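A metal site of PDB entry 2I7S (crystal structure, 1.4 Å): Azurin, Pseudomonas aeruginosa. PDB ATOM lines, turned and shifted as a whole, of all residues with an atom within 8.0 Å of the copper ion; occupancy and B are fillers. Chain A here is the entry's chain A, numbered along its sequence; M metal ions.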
ATOM      1  N   GLY A   9      -4.936  24.264 -26.439  1.00  0.00           N
ATOM      2  CA  GLY A   9      -6.257  24.192 -25.812  1.00  0.00           C
ATOM      3  C   GLY A   9      -6.133  24.601 -24.345  1.00  0.00           C
ATOM      4  O   GLY A   9      -5.310  24.056 -23.603  1.00  0.00           O
ATOM      5  N   ASN A  10      -6.932  25.574 -23.909  1.00  0.00           N
ATOM      6  CA  ASN A  10      -6.805  26.105 -22.564  1.00  0.00           C
ATOM      7  C   ASN A  10      -7.933  25.677 -21.626  1.00  0.00           C
ATOM      8  O   ASN A  10      -8.794  24.859 -21.954  1.00  0.00           O
ATOM      9  CB  ASN A  10      -6.688  27.651 -22.632  1.00  0.00           C
ATOM     10  CG  ASN A  10      -7.982  28.340 -23.035  1.00  0.00           C
ATOM     11  OD1 ASN A  10      -9.042  27.730 -23.139  1.00  0.00           O
ATOM     12  ND2 ASN A  10      -7.958  29.652 -23.272  1.00  0.00           N
ATOM     13  N   MET A  13     -11.832  26.135 -22.556  1.00  0.00           N
ATOM     14  CA  MET A  13     -12.403  25.284 -23.608  1.00  0.00           C
ATOM     15  C   MET A  13     -12.322  25.980 -24.966  1.00  0.00           C
ATOM     16  O   MET A  13     -13.274  25.931 -25.759  1.00  0.00           O
ATOM     17  CB  MET A  13     -13.848  24.856 -23.261  1.00  0.00           C
ATOM     18  CG  MET A  13     -14.366  23.540 -23.808  1.00  0.00           C
ATOM     19  SD  MET A  13     -16.134  23.226 -23.455  1.00  0.00           S
ATOM     20  CE  MET A  13     -16.867  24.327 -24.662  1.00  0.00           C
ATOM     21  N   GLN A  14     -11.185  26.588 -25.254  1.00  0.00           N
ATOM     22  CA  GLN A  14     -10.933  27.219 -26.547  1.00  0.00           C
ATOM     23  C   GLN A  14      -9.614  26.772 -27.178  1.00  0.00           C
ATOM     24  O   GLN A  14      -8.655  26.551 -26.437  1.00  0.00           O
ATOM     25  CB  GLN A  14     -10.834  28.745 -26.481  1.00  0.00           C
ATOM     26  CG  GLN A  14     -12.134  29.405 -26.013  1.00  0.00           C
ATOM     27  CD  GLN A  14     -12.927  30.032 -27.142  1.00  0.00           C
ATOM     28  OE1 GLN A  14     -13.888  30.766 -26.932  1.00  0.00           O
ATOM     29  NE2 GLN A  14     -12.530  29.742 -28.384  1.00  0.00           N
ATOM     30  N   PHE A  15      -9.579  26.652 -28.499  1.00  0.00           N
ATOM     31  CA  PHE A  15      -8.314  26.544 -29.232  1.00  0.00           C
ATOM     32  C   PHE A  15      -7.796  27.974 -29.446  1.00  0.00           C
ATOM     33  O   PHE A  15      -8.621  28.896 -29.414  1.00  0.00           O
ATOM     34  CB  PHE A  15      -8.499  25.828 -30.556  1.00  0.00           C
ATOM     35  CG  PHE A  15      -8.581  24.296 -30.563  1.00  0.00           C
ATOM     36  CD1 PHE A  15      -7.603  23.566 -29.884  1.00  0.00           C
ATOM     37  CD2 PHE A  15      -9.589  23.638 -31.227  1.00  0.00           C
ATOM     38  CE1 PHE A  15      -7.686  22.185 -29.917  1.00  0.00           C
ATOM     39  CE2 PHE A  15      -9.639  22.239 -31.266  1.00  0.00           C
ATOM     40  CZ  PHE A  15      -8.648  21.483 -30.633  1.00  0.00           C
ATOM     41  N   LEU A  33       0.265  20.101 -30.350  1.00  0.00           N
ATOM     42  CA  LEU A  33      -0.739  20.503 -29.388  1.00  0.00           C
ATOM     43  C   LEU A  33      -0.175  20.636 -27.976  1.00  0.00           C
ATOM     44  O   LEU A  33       0.553  19.794 -27.474  1.00  0.00           O
ATOM     45  CB  LEU A  33      -1.909  19.500 -29.423  1.00  0.00           C
ATOM     46  CG  LEU A  33      -3.101  19.769 -28.491  1.00  0.00           C
ATOM     47  CD1 LEU A  33      -3.917  20.973 -28.898  1.00  0.00           C
ATOM     48  CD2 LEU A  33      -4.022  18.542 -28.449  1.00  0.00           C
ATOM     49  N   HIS A  35      -1.334  22.121 -23.723  1.00  0.00           N
ATOM     50  CA  HIS A  35      -2.415  22.513 -22.808  1.00  0.00           C
ATOM     51  C   HIS A  35      -1.883  23.357 -21.662  1.00  0.00           C
ATOM     52  O   HIS A  35      -1.477  22.874 -20.609  1.00  0.00           O
ATOM     53  CB  HIS A  35      -3.097  21.234 -22.329  1.00  0.00           C
ATOM     54  CG  HIS A  35      -4.358  21.384 -21.556  1.00  0.00           C
ATOM     55  ND1 HIS A  35      -4.629  22.460 -20.729  1.00  0.00           N
ATOM     56  CD2 HIS A  35      -5.438  20.552 -21.494  1.00  0.00           C
ATOM     57  CE1 HIS A  35      -5.833  22.278 -20.188  1.00  0.00           C
ATOM     58  NE2 HIS A  35      -6.341  21.128 -20.635  1.00  0.00           N
ATOM     59  N   LYS A  41      -6.951  16.044 -17.433  1.00  0.00           N
ATOM     60  CA  LYS A  41      -7.614  15.620 -18.672  1.00  0.00           C
ATOM     61  C   LYS A  41      -8.981  15.003 -18.452  1.00  0.00           C
ATOM     62  O   LYS A  41      -9.760  14.892 -19.417  1.00  0.00           O
ATOM     63  CB  LYS A  41      -6.712  14.654 -19.454  1.00  0.00           C
ATOM     64  CG  LYS A  41      -6.330  13.364 -18.783  1.00  0.00           C
ATOM     65  CD  LYS A  41      -5.442  12.559 -19.747  1.00  0.00           C
ATOM     66  CE  LYS A  41      -5.083  11.206 -19.122  1.00  0.00           C
ATOM     67  NZ  LYS A  41      -4.010  10.512 -19.880  1.00  0.00           N
ATOM     68  N   VAL A  43     -11.410  16.303 -16.763  1.00  0.00           N
ATOM     69  CA  VAL A  43     -12.416  17.377 -16.758  1.00  0.00           C
ATOM     70  C   VAL A  43     -12.133  18.449 -17.792  1.00  0.00           C
ATOM     71  O   VAL A  43     -13.038  19.214 -18.091  1.00  0.00           O
ATOM     72  CB  VAL A  43     -12.511  18.054 -15.377  1.00  0.00           C
ATOM     73  CG1 VAL A  43     -12.880  17.044 -14.292  1.00  0.00           C
ATOM     74  CG2 VAL A  43     -11.208  18.720 -15.006  1.00  0.00           C
ATOM     75  N   MET A  44     -10.926  18.476 -18.356  1.00  0.00           N
ATOM     76  CA  MET A  44     -10.639  19.495 -19.391  1.00  0.00           C
ATOM     77  C   MET A  44      -9.650  18.953 -20.402  1.00  0.00           C
ATOM     78  O   MET A  44      -8.762  19.664 -20.852  1.00  0.00           O
ATOM     79  CB  MET A  44     -10.163  20.790 -18.759  1.00  0.00           C
ATOM     80  CG  MET A  44     -10.059  22.031 -19.620  1.00  0.00           C
ATOM     81  SD  MET A  44     -11.515  22.443 -20.593  1.00  0.00           S
ATOM     82  CE  MET A  44     -12.709  22.855 -19.324  1.00  0.00           C
ATOM     83  N   GLY A  45      -9.813  17.674 -20.785  1.00  0.00           N
ATOM     84  CA  GLY A  45      -8.896  17.085 -21.753  1.00  0.00           C
ATOM     85  C   GLY A  45      -9.106  17.641 -23.157  1.00  0.00           C
ATOM     86  O   GLY A  45     -10.237  17.987 -23.544  1.00  0.00           O
ATOM     87  N   HIS A  46      -8.005  17.736 -23.913  1.00  0.00           N
ATOM     88  CA  HIS A  46      -8.087  18.166 -25.305  1.00  0.00           C
ATOM     89  C   HIS A  46      -7.282  17.262 -26.225  1.00  0.00           C
ATOM     90  O   HIS A  46      -6.193  16.816 -25.843  1.00  0.00           O
ATOM     91  CB  HIS A  46      -7.592  19.607 -25.460  1.00  0.00           C
ATOM     92  CG  HIS A  46      -8.297  20.656 -24.672  1.00  0.00           C
ATOM     93  ND1 HIS A  46      -9.658  20.800 -24.594  1.00  0.00           N
ATOM     94  CD2 HIS A  46      -7.739  21.635 -23.912  1.00  0.00           C
ATOM     95  CE1 HIS A  46      -9.919  21.830 -23.807  1.00  0.00           C
ATOM     96  NE2 HIS A  46      -8.774  22.373 -23.377  1.00  0.00           N
ATOM     97  N   ASN A  47      -7.876  16.976 -27.385  1.00  0.00           N
ATOM     98  CA  ASN A  47      -7.156  16.356 -28.506  1.00  0.00           C
ATOM     99  C   ASN A  47      -7.357  17.260 -29.726  1.00  0.00           C
ATOM    100  O   ASN A  47      -8.119  18.231 -29.633  1.00  0.00           O
ATOM    101  CB  ASN A  47      -7.533  14.912 -28.791  1.00  0.00           C
ATOM    102  CG  ASN A  47      -9.026  14.714 -28.951  1.00  0.00           C
ATOM    103  OD1 ASN A  47      -9.810  15.597 -29.310  1.00  0.00           O
ATOM    104  ND2 ASN A  47      -9.510  13.509 -28.669  1.00  0.00           N
ATOM    105  N   TRP A  48      -6.661  16.936 -30.793  1.00  0.00           N
ATOM    106  CA  TRP A  48      -6.748  17.607 -32.088  1.00  0.00           C
ATOM    107  C   TRP A  48      -7.038  16.485 -33.098  1.00  0.00           C
ATOM    108  O   TRP A  48      -6.212  15.573 -33.273  1.00  0.00           O
ATOM    109  CB  TRP A  48      -5.512  18.429 -32.416  1.00  0.00           C
ATOM    110  CG  TRP A  48      -5.603  19.221 -33.700  1.00  0.00           C
ATOM    111  CD1 TRP A  48      -5.985  20.548 -33.776  1.00  0.00           C
ATOM    112  CD2 TRP A  48      -5.325  18.797 -35.038  1.00  0.00           C
ATOM    113  NE1 TRP A  48      -5.955  20.941 -35.082  1.00  0.00           N
ATOM    114  CE2 TRP A  48      -5.552  19.908 -35.899  1.00  0.00           C
ATOM    115  CE3 TRP A  48      -4.899  17.601 -35.637  1.00  0.00           C
ATOM    116  CZ2 TRP A  48      -5.371  19.841 -37.273  1.00  0.00           C
ATOM    117  CZ3 TRP A  48      -4.730  17.546 -37.013  1.00  0.00           C
ATOM    118  CH2 TRP A  48      -4.969  18.658 -37.843  1.00  0.00           C
ATOM    119  N   TYR A  72     -11.545   9.382 -25.937  1.00  0.00           N
ATOM    120  CA  TYR A  72     -12.798   9.834 -26.546  1.00  0.00           C
ATOM    121  C   TYR A  72     -12.724   9.751 -28.073  1.00  0.00           C
ATOM    122  O   TYR A  72     -13.214  10.645 -28.756  1.00  0.00           O
ATOM    123  CB  TYR A  72     -13.139  11.243 -26.067  1.00  0.00           C
ATOM    124  CG  TYR A  72     -13.589  11.276 -24.616  1.00  0.00           C
ATOM    125  CD1 TYR A  72     -14.771  10.670 -24.243  1.00  0.00           C
ATOM    126  CD2 TYR A  72     -12.849  11.946 -23.645  1.00  0.00           C
ATOM    127  CE1 TYR A  72     -15.222  10.705 -22.933  1.00  0.00           C
ATOM    128  CE2 TYR A  72     -13.285  11.981 -22.322  1.00  0.00           C
ATOM    129  CZ  TYR A  72     -14.467  11.352 -21.993  1.00  0.00           C
ATOM    130  OH  TYR A  72     -14.879  11.399 -20.684  1.00  0.00           O
ATOM    131  N   LEU A  86      -5.391  12.443 -26.108  1.00  0.00           N
ATOM    132  CA  LEU A  86      -6.073  13.398 -25.230  1.00  0.00           C
ATOM    133  C   LEU A  86      -5.114  13.870 -24.148  1.00  0.00           C
ATOM    134  O   LEU A  86      -4.529  13.014 -23.456  1.00  0.00           O
ATOM    135  CB  LEU A  86      -7.316  12.739 -24.606  1.00  0.00           C
ATOM    136  CG  LEU A  86      -8.258  13.662 -23.853  1.00  0.00           C
ATOM    137  CD1 LEU A  86      -9.222  14.395 -24.800  1.00  0.00           C
ATOM    138  CD2 LEU A  86      -9.016  12.912 -22.772  1.00  0.00           C
ATOM    139  N   ILE A  87      -4.916  15.174 -23.981  1.00  0.00           N
ATOM    140  CA  ILE A  87      -3.946  15.690 -22.994  1.00  0.00           C
ATOM    141  C   ILE A  87      -4.595  16.588 -21.964  1.00  0.00           C
ATOM    142  O   ILE A  87      -5.623  17.206 -22.260  1.00  0.00           O
ATOM    143  CB  ILE A  87      -2.822  16.468 -23.718  1.00  0.00           C
ATOM    144  CG1 ILE A  87      -3.304  17.637 -24.573  1.00  0.00           C
ATOM    145  CG2 ILE A  87      -1.966  15.499 -24.537  1.00  0.00           C
ATOM    146  CD1 ILE A  87      -2.163  18.583 -24.969  1.00  0.00           C
ATOM    147  N   PHE A 111     -11.050  19.526 -34.634  1.00  0.00           N
ATOM    148  CA  PHE A 111     -11.903  19.647 -33.457  1.00  0.00           C
ATOM    149  C   PHE A 111     -11.376  18.800 -32.304  1.00  0.00           C
ATOM    150  O   PHE A 111     -10.560  17.892 -32.546  1.00  0.00           O
ATOM    151  CB  PHE A 111     -13.346  19.223 -33.848  1.00  0.00           C
ATOM    152  CG  PHE A 111     -13.433  17.926 -34.604  1.00  0.00           C
ATOM    153  CD1 PHE A 111     -13.397  17.902 -35.995  1.00  0.00           C
ATOM    154  CD2 PHE A 111     -13.539  16.696 -33.960  1.00  0.00           C
ATOM    155  CE1 PHE A 111     -13.493  16.729 -36.733  1.00  0.00           C
ATOM    156  CE2 PHE A 111     -13.593  15.513 -34.670  1.00  0.00           C
ATOM    157  CZ  PHE A 111     -13.541  15.530 -36.052  1.00  0.00           C
ATOM    158  N   CYS A 112     -11.817  19.091 -31.087  1.00  0.00           N
ATOM    159  CA  CYS A 112     -11.606  18.274 -29.884  1.00  0.00           C
ATOM    160  C   CYS A 112     -12.825  17.380 -29.649  1.00  0.00           C
ATOM    161  O   CYS A 112     -13.949  17.861 -29.756  1.00  0.00           O
ATOM    162  CB  CYS A 112     -11.321  19.158 -28.647  1.00  0.00           C
ATOM    163  SG  CYS A 112     -11.174  18.215 -27.122  1.00  0.00           S
ATOM    164  N   THR A 113     -12.593  16.104 -29.348  1.00  0.00           N
ATOM    165  CA  THR A 113     -13.732  15.186 -29.144  1.00  0.00           C
ATOM    166  C   THR A 113     -14.054  14.948 -27.671  1.00  0.00           C
ATOM    167  O   THR A 113     -14.927  14.100 -27.355  1.00  0.00           O
ATOM    168  CB  THR A 113     -13.541  13.809 -29.821  1.00  0.00           C
ATOM    169  OG1 THR A 113     -12.375  13.188 -29.267  1.00  0.00           O
ATOM    170  CG2 THR A 113     -13.309  13.894 -31.331  1.00  0.00           C
ATOM    171  N   PHE A 114     -13.463  15.673 -26.712  1.00  0.00           N
ATOM    172  CA  PHE A 114     -13.896  15.512 -25.299  1.00  0.00           C
ATOM    173  C   PHE A 114     -15.327  15.955 -25.221  1.00  0.00           C
ATOM    174  O   PHE A 114     -15.680  16.955 -25.890  1.00  0.00           O
ATOM    175  CB  PHE A 114     -12.990  16.347 -24.384  1.00  0.00           C
ATOM    176  CG  PHE A 114     -13.302  16.221 -22.883  1.00  0.00           C
ATOM    177  CD1 PHE A 114     -14.385  16.892 -22.317  1.00  0.00           C
ATOM    178  CD2 PHE A 114     -12.514  15.409 -22.064  1.00  0.00           C
ATOM    179  CE1 PHE A 114     -14.665  16.785 -20.951  1.00  0.00           C
ATOM    180  CE2 PHE A 114     -12.786  15.308 -20.708  1.00  0.00           C
ATOM    181  CZ  PHE A 114     -13.859  15.994 -20.155  1.00  0.00           C
ATOM    182  N   PRO A 115     -16.222  15.302 -24.469  1.00  0.00           N
ATOM    183  CA  PRO A 115     -17.650  15.649 -24.498  1.00  0.00           C
ATOM    184  C   PRO A 115     -17.955  17.138 -24.303  1.00  0.00           C
ATOM    185  O   PRO A 115     -17.580  17.796 -23.346  1.00  0.00           O
ATOM    186  CB  PRO A 115     -18.210  14.813 -23.336  1.00  0.00           C
ATOM    187  CG  PRO A 115     -17.338  13.586 -23.371  1.00  0.00           C
ATOM    188  CD  PRO A 115     -15.932  14.179 -23.575  1.00  0.00           C
ATOM    189  N   GLY A 116     -18.664  17.680 -25.308  1.00  0.00           N
ATOM    190  CA  GLY A 116     -19.113  19.067 -25.371  1.00  0.00           C
ATOM    191  C   GLY A 116     -18.115  20.021 -26.004  1.00  0.00           C
ATOM    192  O   GLY A 116     -18.405  21.161 -26.445  1.00  0.00           O
ATOM    193  N   HIS A 117     -16.837  19.635 -26.058  1.00  0.00           N
ATOM    194  CA  HIS A 117     -15.852  20.657 -26.398  1.00  0.00           C
ATOM    195  C   HIS A 117     -15.951  21.155 -27.821  1.00  0.00           C
ATOM    196  O   HIS A 117     -15.678  22.345 -28.067  1.00  0.00           O
ATOM    197  CB  HIS A 117     -14.412  20.123 -26.134  1.00  0.00           C
ATOM    198  CG  HIS A 117     -14.048  20.105 -24.674  1.00  0.00           C
ATOM    199  ND1 HIS A 117     -12.750  19.995 -24.208  1.00  0.00           N
ATOM    200  CD2 HIS A 117     -14.844  20.172 -23.576  1.00  0.00           C
ATOM    201  CE1 HIS A 117     -12.750  20.003 -22.890  1.00  0.00           C
ATOM    202  NE2 HIS A 117     -14.018  20.115 -22.467  1.00  0.00           N
ATOM    203  N   SER A 118     -16.340  20.320 -28.779  1.00  0.00           N
ATOM    204  CA  SER A 118     -16.359  20.781 -30.172  1.00  0.00           C
ATOM    205  C   SER A 118     -17.330  21.928 -30.435  1.00  0.00           C
ATOM    206  O   SER A 118     -17.274  22.529 -31.521  1.00  0.00           O
ATOM    207  CB  SER A 118     -16.677  19.609 -31.113  1.00  0.00           C
ATOM    208  OG  SER A 118     -17.945  19.006 -30.856  1.00  0.00           O
ATOM    209  N   MET A 121     -14.501  24.248 -29.754  1.00  0.00           N
ATOM    210  CA  MET A 121     -13.188  23.778 -30.142  1.00  0.00           C
ATOM    211  C   MET A 121     -13.231  23.053 -31.481  1.00  0.00           C
ATOM    212  O   MET A 121     -13.193  21.822 -31.576  1.00  0.00           O
ATOM    213  CB  MET A 121     -12.633  22.865 -29.019  1.00  0.00           C
ATOM    214  CG  MET A 121     -12.365  23.648 -27.737  1.00  0.00           C
ATOM    215  SD  MET A 121     -11.443  22.720 -26.474  1.00  0.00           S
ATOM    216  CE  MET A 121      -9.787  22.860 -27.164  1.00  0.00           C
HETATM  217 CU    CU M   1     -11.042  19.528 -25.276  1.00  0.00          CU
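The copper ion is bound by a ring nitrogen (ND1) of His 46, at 2.0 Å.
ND1 of His 117 is bound to the copper ion (2.1 Å).
The side-chain sulfur (SG) of Cys 112 is bound to the copper ion.
The backbone carbonyl oxygen (O) of Gly 45 binds the copper ion, at 2.5 Å.
The copper ion has four donor atoms within binding distance.
Merely in contact with the copper ion: Met 121 (3.4 Å) and Phe 114 (3.8 Å).
Six residues have an atom within 4 Å of the copper ion: Gly 45, His 46, Cys 112, Phe 114, His 117 and Met 121.
The nearest printed residue that does not touch the copper ion is Asn 47 (4.6 Å).
A ring nitrogen (ND1) of His 46 lies close to the side-chain sulfur (SD) of Met 121 (3.2 Å).
The backbone NH (N) of Ile 87 lies within hydrogen-bond range of the backbone carbonyl oxygen (O) of His 46 (2.8 Å).
NE2 of His 46 is in hydrogen-bond range of O of Asn 10 (2.9 Å).
The side-chain sulfur (SD) of Met 121 sits close to a ring nitrogen (ND1) of His 117, 3.8 Å away.
O of Met 121 is in hydrogen-bond range of N of Cys 112 (3.1 Å).
The side-chain sulfur of Cys 112 lies close to the backbone NH of Phe 114 (3.4 Å).
The side-chain sulfur (SG) of Cys 112 lies close to the backbone NH (N) of Asn 47, 3.5 Å away.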
